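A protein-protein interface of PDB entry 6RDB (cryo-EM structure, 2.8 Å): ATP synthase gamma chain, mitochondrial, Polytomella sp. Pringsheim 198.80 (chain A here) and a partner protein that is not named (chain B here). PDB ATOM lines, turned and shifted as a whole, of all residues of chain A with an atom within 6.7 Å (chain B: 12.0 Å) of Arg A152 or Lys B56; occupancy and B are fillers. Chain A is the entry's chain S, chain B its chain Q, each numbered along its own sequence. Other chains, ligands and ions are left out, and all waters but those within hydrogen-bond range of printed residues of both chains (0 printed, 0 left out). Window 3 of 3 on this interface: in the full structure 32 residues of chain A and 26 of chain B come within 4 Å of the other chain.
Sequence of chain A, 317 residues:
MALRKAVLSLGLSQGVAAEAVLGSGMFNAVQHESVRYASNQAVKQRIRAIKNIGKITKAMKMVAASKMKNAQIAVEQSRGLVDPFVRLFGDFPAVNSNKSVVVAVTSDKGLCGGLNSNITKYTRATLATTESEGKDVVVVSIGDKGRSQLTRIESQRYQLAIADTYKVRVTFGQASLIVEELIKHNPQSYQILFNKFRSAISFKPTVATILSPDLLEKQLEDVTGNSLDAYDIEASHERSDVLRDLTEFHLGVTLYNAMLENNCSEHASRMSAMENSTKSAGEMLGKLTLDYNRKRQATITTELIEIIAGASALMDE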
ATOM      1  N   ARG A 147      12.643  27.458  11.075  1.00  0.00           N
ATOM      2  CA  ARG A 147      13.184  26.674  12.176  1.00  0.00           C
ATOM      3  C   ARG A 147      14.523  27.209  12.657  1.00  0.00           C
ATOM      4  O   ARG A 147      14.911  26.941  13.799  1.00  0.00           O
ATOM      5  CB  ARG A 147      13.329  25.212  11.762  1.00  0.00           C
ATOM      6  CG  ARG A 147      14.148  25.004  10.512  1.00  0.00           C
ATOM      7  CD  ARG A 147      14.803  23.638  10.517  1.00  0.00           C
ATOM      8  NE  ARG A 147      15.853  23.528   9.508  1.00  0.00           N
ATOM      9  CZ  ARG A 147      17.109  23.922   9.693  1.00  0.00           C
ATOM     10  NH1 ARG A 147      17.999  23.783   8.723  1.00  0.00           N
ATOM     11  NH2 ARG A 147      17.475  24.459  10.847  1.00  0.00           N
ATOM     12  N   SER A 148      15.232  27.953  11.814  1.00  0.00           N
ATOM     13  CA  SER A 148      16.505  28.539  12.194  1.00  0.00           C
ATOM     14  C   SER A 148      16.351  29.877  12.899  1.00  0.00           C
ATOM     15  O   SER A 148      17.329  30.374  13.466  1.00  0.00           O
ATOM     16  CB  SER A 148      17.385  28.702  10.956  1.00  0.00           C
ATOM     17  OG  SER A 148      17.327  27.539  10.150  1.00  0.00           O
ATOM     18  N   GLN A 149      15.161  30.473  12.876  1.00  0.00           N
ATOM     19  CA  GLN A 149      14.946  31.764  13.507  1.00  0.00           C
ATOM     20  C   GLN A 149      13.919  31.746  14.624  1.00  0.00           C
ATOM     21  O   GLN A 149      13.952  32.640  15.476  1.00  0.00           O
ATOM     22  CB  GLN A 149      14.520  32.811  12.466  1.00  0.00           C
ATOM     23  CG  GLN A 149      15.407  32.839  11.242  1.00  0.00           C
ATOM     24  CD  GLN A 149      15.078  33.976  10.315  1.00  0.00           C
ATOM     25  OE1 GLN A 149      14.582  35.017  10.743  1.00  0.00           O
ATOM     26  NE2 GLN A 149      15.357  33.789   9.033  1.00  0.00           N
ATOM     27  N   LEU A 150      13.016  30.768  14.651  1.00  0.00           N
ATOM     28  CA  LEU A 150      12.074  30.677  15.758  1.00  0.00           C
ATOM     29  C   LEU A 150      12.696  30.001  16.970  1.00  0.00           C
ATOM     30  O   LEU A 150      12.291  30.283  18.103  1.00  0.00           O
ATOM     31  CB  LEU A 150      10.812  29.933  15.322  1.00  0.00           C
ATOM     32  CG  LEU A 150       9.845  30.723  14.439  1.00  0.00           C
ATOM     33  CD1 LEU A 150       8.771  29.818  13.906  1.00  0.00           C
ATOM     34  CD2 LEU A 150       9.222  31.869  15.209  1.00  0.00           C
ATOM     35  N   THR A 151      13.681  29.122  16.749  1.00  0.00           N
ATOM     36  CA  THR A 151      14.428  28.521  17.850  1.00  0.00           C
ATOM     37  C   THR A 151      15.217  29.571  18.628  1.00  0.00           C
ATOM     38  O   THR A 151      15.348  29.470  19.853  1.00  0.00           O
ATOM     39  CB  THR A 151      15.350  27.429  17.296  1.00  0.00           C
ATOM     40  OG1 THR A 151      14.579  26.518  16.504  1.00  0.00           O
ATOM     41  CG2 THR A 151      16.025  26.645  18.408  1.00  0.00           C
ATOM     42  N   ARG A 152      15.709  30.607  17.941  1.00  0.00           N
ATOM     43  CA  ARG A 152      16.402  31.708  18.606  1.00  0.00           C
ATOM     44  C   ARG A 152      15.480  32.536  19.492  1.00  0.00           C
ATOM     45  O   ARG A 152      15.944  33.112  20.480  1.00  0.00           O
ATOM     46  CB  ARG A 152      17.053  32.636  17.573  1.00  0.00           C
ATOM     47  CG  ARG A 152      17.910  31.947  16.519  1.00  0.00           C
ATOM     48  CD  ARG A 152      19.324  31.711  17.019  1.00  0.00           C
ATOM     49  NE  ARG A 152      19.430  30.463  17.766  1.00  0.00           N
ATOM     50  CZ  ARG A 152      19.675  29.281  17.212  1.00  0.00           C
ATOM     51  NH1 ARG A 152      19.749  28.196  17.969  1.00  0.00           N
ATOM     52  NH2 ARG A 152      19.855  29.183  15.903  1.00  0.00           N
ATOM     53  N   ILE A 153      14.198  32.613  19.160  1.00  0.00           N
ATOM     54  CA  ILE A 153      13.252  33.462  19.873  1.00  0.00           C
ATOM     55  C   ILE A 153      12.415  32.660  20.859  1.00  0.00           C
ATOM     56  O   ILE A 153      12.260  33.048  22.017  1.00  0.00           O
ATOM     57  CB  ILE A 153      12.370  34.225  18.858  1.00  0.00           C
ATOM     58  CG1 ILE A 153      13.157  35.385  18.244  1.00  0.00           C
ATOM     59  CG2 ILE A 153      11.070  34.707  19.490  1.00  0.00           C
ATOM     60  CD1 ILE A 153      13.568  36.446  19.238  1.00  0.00           C
ATOM     61  N   GLU A 154      11.893  31.514  20.425  1.00  0.00           N
ATOM     62  CA  GLU A 154      10.964  30.753  21.252  1.00  0.00           C
ATOM     63  C   GLU A 154      11.102  29.288  20.842  1.00  0.00           C
ATOM     64  O   GLU A 154      10.488  28.859  19.863  1.00  0.00           O
ATOM     65  CB  GLU A 154       9.546  31.276  21.058  1.00  0.00           C
ATOM     66  CG  GLU A 154       8.672  31.207  22.285  1.00  0.00           C
ATOM     67  CD  GLU A 154       8.284  29.805  22.655  1.00  0.00           C
ATOM     68  OE1 GLU A 154       8.032  29.572  23.851  1.00  0.00           O
ATOM     69  OE2 GLU A 154       8.190  28.953  21.750  1.00  0.00           O
ATOM     70  N   SER A 155      11.888  28.528  21.603  1.00  0.00           N
ATOM     71  CA  SER A 155      12.236  27.162  21.235  1.00  0.00           C
ATOM     72  C   SER A 155      11.540  26.094  22.062  1.00  0.00           C
ATOM     73  O   SER A 155      11.319  24.993  21.558  1.00  0.00           O
ATOM     74  CB  SER A 155      13.751  26.950  21.351  1.00  0.00           C
ATOM     75  OG  SER A 155      14.097  25.614  21.039  1.00  0.00           O
ATOM     76  N   TYR A 158       8.097  25.224  20.747  1.00  0.00           N
ATOM     77  CA  TYR A 158       8.182  24.955  19.320  1.00  0.00           C
ATOM     78  C   TYR A 158       8.080  23.450  19.109  1.00  0.00           C
ATOM     79  O   TYR A 158       8.762  22.686  19.795  1.00  0.00           O
ATOM     80  CB  TYR A 158       9.501  25.502  18.769  1.00  0.00           C
ATOM     81  CG  TYR A 158       9.703  25.335  17.285  1.00  0.00           C
ATOM     82  CD1 TYR A 158      10.436  24.271  16.788  1.00  0.00           C
ATOM     83  CD2 TYR A 158       9.187  26.256  16.385  1.00  0.00           C
ATOM     84  CE1 TYR A 158      10.633  24.111  15.437  1.00  0.00           C
ATOM     85  CE2 TYR A 158       9.378  26.104  15.026  1.00  0.00           C
ATOM     86  CZ  TYR A 158      10.103  25.029  14.562  1.00  0.00           C
ATOM     87  OH  TYR A 158      10.303  24.864  13.216  1.00  0.00           O
ATOM     88  N   ARG B  48       7.759  18.283   3.260  1.00  0.00           N
ATOM     89  CA  ARG B  48       8.332  17.421   4.280  1.00  0.00           C
ATOM     90  C   ARG B  48       8.048  18.043   5.636  1.00  0.00           C
ATOM     91  O   ARG B  48       7.765  19.237   5.742  1.00  0.00           O
ATOM     92  CB  ARG B  48       9.838  17.212   4.068  1.00  0.00           C
ATOM     93  CG  ARG B  48      10.695  18.441   4.308  1.00  0.00           C
ATOM     94  CD  ARG B  48      12.173  18.105   4.249  1.00  0.00           C
ATOM     95  NE  ARG B  48      12.909  18.771   5.319  1.00  0.00           N
ATOM     96  CZ  ARG B  48      13.597  19.897   5.168  1.00  0.00           C
ATOM     97  NH1 ARG B  48      14.225  20.432   6.204  1.00  0.00           N
ATOM     98  NH2 ARG B  48      13.658  20.490   3.984  1.00  0.00           N
ATOM     99  N   GLN B  49       8.107  17.218   6.678  1.00  0.00           N
ATOM    100  CA  GLN B  49       7.820  17.689   8.024  1.00  0.00           C
ATOM    101  C   GLN B  49       8.779  17.038   9.006  1.00  0.00           C
ATOM    102  O   GLN B  49       9.426  16.032   8.704  1.00  0.00           O
ATOM    103  CB  GLN B  49       6.367  17.408   8.432  1.00  0.00           C
ATOM    104  CG  GLN B  49       6.118  15.999   8.915  1.00  0.00           C
ATOM    105  CD  GLN B  49       4.651  15.690   9.090  1.00  0.00           C
ATOM    106  OE1 GLN B  49       4.008  15.143   8.194  1.00  0.00           O
ATOM    107  NE2 GLN B  49       4.109  16.036  10.251  1.00  0.00           N
ATOM    108  N   ALA B  50       8.863  17.632  10.197  1.00  0.00           N
ATOM    109  CA  ALA B  50       9.766  17.183  11.225  1.00  0.00           C
ATOM    110  C   ALA B  50       9.249  17.670  12.570  1.00  0.00           C
ATOM    111  O   ALA B  50       9.013  18.878  12.726  1.00  0.00           O
ATOM    112  CB  ALA B  50      11.184  17.701  10.997  1.00  0.00           C
ATOM    113  N   PRO B  51       9.048  16.780  13.538  1.00  0.00           N
ATOM    114  CA  PRO B  51       8.675  17.224  14.882  1.00  0.00           C
ATOM    115  C   PRO B  51       9.870  17.800  15.616  1.00  0.00           C
ATOM    116  O   PRO B  51      11.023  17.512  15.297  1.00  0.00           O
ATOM    117  CB  PRO B  51       8.179  15.940  15.558  1.00  0.00           C
ATOM    118  CG  PRO B  51       8.004  14.942  14.446  1.00  0.00           C
ATOM    119  CD  PRO B  51       9.005  15.316  13.414  1.00  0.00           C
ATOM    120  N   TYR B  52       9.581  18.634  16.613  1.00  0.00           N
ATOM    121  CA  TYR B  52      10.614  19.261  17.443  1.00  0.00           C
ATOM    122  C   TYR B  52      10.192  19.094  18.898  1.00  0.00           C
ATOM    123  O   TYR B  52       9.507  19.950  19.459  1.00  0.00           O
ATOM    124  CB  TYR B  52      10.806  20.726  17.072  1.00  0.00           C
ATOM    125  CG  TYR B  52      11.893  20.975  16.050  1.00  0.00           C
ATOM    126  CD1 TYR B  52      13.067  21.626  16.401  1.00  0.00           C
ATOM    127  CD2 TYR B  52      11.738  20.569  14.730  1.00  0.00           C
ATOM    128  CE1 TYR B  52      14.065  21.857  15.466  1.00  0.00           C
ATOM    129  CE2 TYR B  52      12.728  20.791  13.792  1.00  0.00           C
ATOM    130  CZ  TYR B  52      13.888  21.435  14.165  1.00  0.00           C
ATOM    131  OH  TYR B  52      14.872  21.662  13.230  1.00  0.00           O
ATOM    132  N   VAL B  53      10.607  17.993  19.516  1.00  0.00           N
ATOM    133  CA  VAL B  53      10.183  17.714  20.883  1.00  0.00           C
ATOM    134  C   VAL B  53      11.087  18.374  21.921  1.00  0.00           C
ATOM    135  O   VAL B  53      10.616  18.736  23.003  1.00  0.00           O
ATOM    136  CB  VAL B  53      10.081  16.193  21.109  1.00  0.00           C
ATOM    137  CG1 VAL B  53       8.939  15.620  20.290  1.00  0.00           C
ATOM    138  CG2 VAL B  53      11.382  15.496  20.735  1.00  0.00           C
ATOM    139  N   ASP B  54      12.370  18.562  21.617  1.00  0.00           N
ATOM    140  CA  ASP B  54      13.309  19.125  22.577  1.00  0.00           C
ATOM    141  C   ASP B  54      13.748  20.538  22.242  1.00  0.00           C
ATOM    142  O   ASP B  54      14.096  21.291  23.152  1.00  0.00           O
ATOM    143  CB  ASP B  54      14.550  18.229  22.695  1.00  0.00           C
ATOM    144  CG  ASP B  54      15.311  18.114  21.392  1.00  0.00           C
ATOM    145  OD1 ASP B  54      16.558  18.164  21.419  1.00  0.00           O
ATOM    146  OD2 ASP B  54      14.655  17.998  20.339  1.00  0.00           O
ATOM    147  N   GLY B  55      13.731  20.918  20.970  1.00  0.00           N
ATOM    148  CA  GLY B  55      14.130  22.255  20.587  1.00  0.00           C
ATOM    149  C   GLY B  55      15.015  22.300  19.359  1.00  0.00           C
ATOM    150  O   GLY B  55      14.981  23.280  18.609  1.00  0.00           O
ATOM    151  N   LYS B  56      15.823  21.262  19.143  1.00  0.00           N
ATOM    152  CA  LYS B  56      16.726  21.262  17.999  1.00  0.00           C
ATOM    153  C   LYS B  56      16.711  19.918  17.276  1.00  0.00           C
ATOM    154  O   LYS B  56      16.970  19.847  16.069  1.00  0.00           O
ATOM    155  CB  LYS B  56      18.139  21.632  18.466  1.00  0.00           C
ATOM    156  CG  LYS B  56      19.175  21.801  17.365  1.00  0.00           C
ATOM    157  CD  LYS B  56      18.781  22.902  16.394  1.00  0.00           C
ATOM    158  CE  LYS B  56      18.853  24.273  17.031  1.00  0.00           C
ATOM    159  NZ  LYS B  56      18.521  25.340  16.046  1.00  0.00           N
ATOM    160  N   ALA B  57      16.370  18.852  17.987  1.00  0.00           N
ATOM    161  CA  ALA B  57      16.400  17.512  17.419  1.00  0.00           C
ATOM    162  C   ALA B  57      14.998  17.084  17.009  1.00  0.00           C
ATOM    163  O   ALA B  57      14.008  17.542  17.587  1.00  0.00           O
ATOM    164  CB  ALA B  57      16.986  16.514  18.417  1.00  0.00           C
ATOM    165  N   GLY B  58      14.915  16.221  15.997  1.00  0.00           N
ATOM    166  CA  GLY B  58      13.651  15.630  15.615  1.00  0.00           C
ATOM    167  C   GLY B  58      13.816  14.626  14.493  1.00  0.00           C
ATOM    168  O   GLY B  58      14.810  14.635  13.765  1.00  0.00           O
ATOM    169  N   ALA B  59      12.804  13.769  14.357  1.00  0.00           N
ATOM    170  CA  ALA B  59      12.773  12.781  13.287  1.00  0.00           C
ATOM    171  C   ALA B  59      12.238  13.425  12.016  1.00  0.00           C
ATOM    172  O   ALA B  59      11.938  14.621  12.008  1.00  0.00           O
ATOM    173  CB  ALA B  59      11.919  11.579  13.688  1.00  0.00           C
ATOM    174  N   SER B  60      12.094  12.654  10.943  1.00  0.00           N
ATOM    175  CA  SER B  60      11.761  13.266   9.666  1.00  0.00           C
ATOM    176  C   SER B  60      10.609  12.520   9.014  1.00  0.00           C
ATOM    177  O   SER B  60      10.256  11.411   9.420  1.00  0.00           O
ATOM    178  CB  SER B  60      12.970  13.296   8.726  1.00  0.00           C
ATOM    179  OG  SER B  60      12.614  13.850   7.471  1.00  0.00           O
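Arg A152 touches one residue of chain B.
Of the printed residues of chain A, Lys B56 touches Thr A151 and Arg A152.
No residue of chain B comes within 4 Å of Ser A148.
No residue of chain B comes within 4 Å of Ile A153.
Ser A155 touches one residue of chain B.
Of the printed residues of chain B, Arg A147 touches Tyr B52 (3.4 Å).
Of the printed residues of chain A, Tyr B52 touches Arg A147 (3.4 Å) and Tyr A158 (2.9 Å).
Printed residues of chain A within 4 Å of Gly B55: Thr A151 (3.5 Å) and Ser A155 (3.4 Å).
Leu A150 touches none of the printed residues of chain B.
Asp B54 touches none of the printed residues of chain A.
The nearest residue of chain B that does not touch Arg A152 is Gly B55 (6.9 Å).
Tyr B52 touches Arg A147 (OH to CD, 3.4 Å).
Thr A151 touches Gly B55.
CG2 of Thr A151 touches NZ of Lys B56, 3.7 Å away.
Arg A152 touches Lys B56 (NH1 to NZ, 3.7 Å).
The side-chain hydroxyl (OG1) of Thr A151 sits at hydrogen-bond distance from the backbone carbonyl oxygen (O) of Arg A147.
The side-chain hydroxyl (OG) of Ser A148 sits at hydrogen-bond distance from the guanidinium group (NH2) of Arg A147, at 3.2 Å.
The backbone carbonyl oxygen of Gly B55 lies close to the side-chain hydroxyl of Ser A155 (3.5 Å).
The backbone carbonyl oxygen (O) of Tyr A158 lies close to the backbone carbonyl oxygen (O) of Tyr B52 (2.9 Å).
Printed residues of chain B that touch a printed residue of chain A: Tyr B52, Gly B55 and Lys B56.
Hydrophobic or aromatic side chains of chain B within 4 Å of the printed part of chain A: Tyr B52.
Printed residues of chain A that touch a printed residue of chain B: Arg A147, Thr A151, Arg A152, Ser A155 and Tyr A158.
Among the printed residues, 6 pairs touch across the chains.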
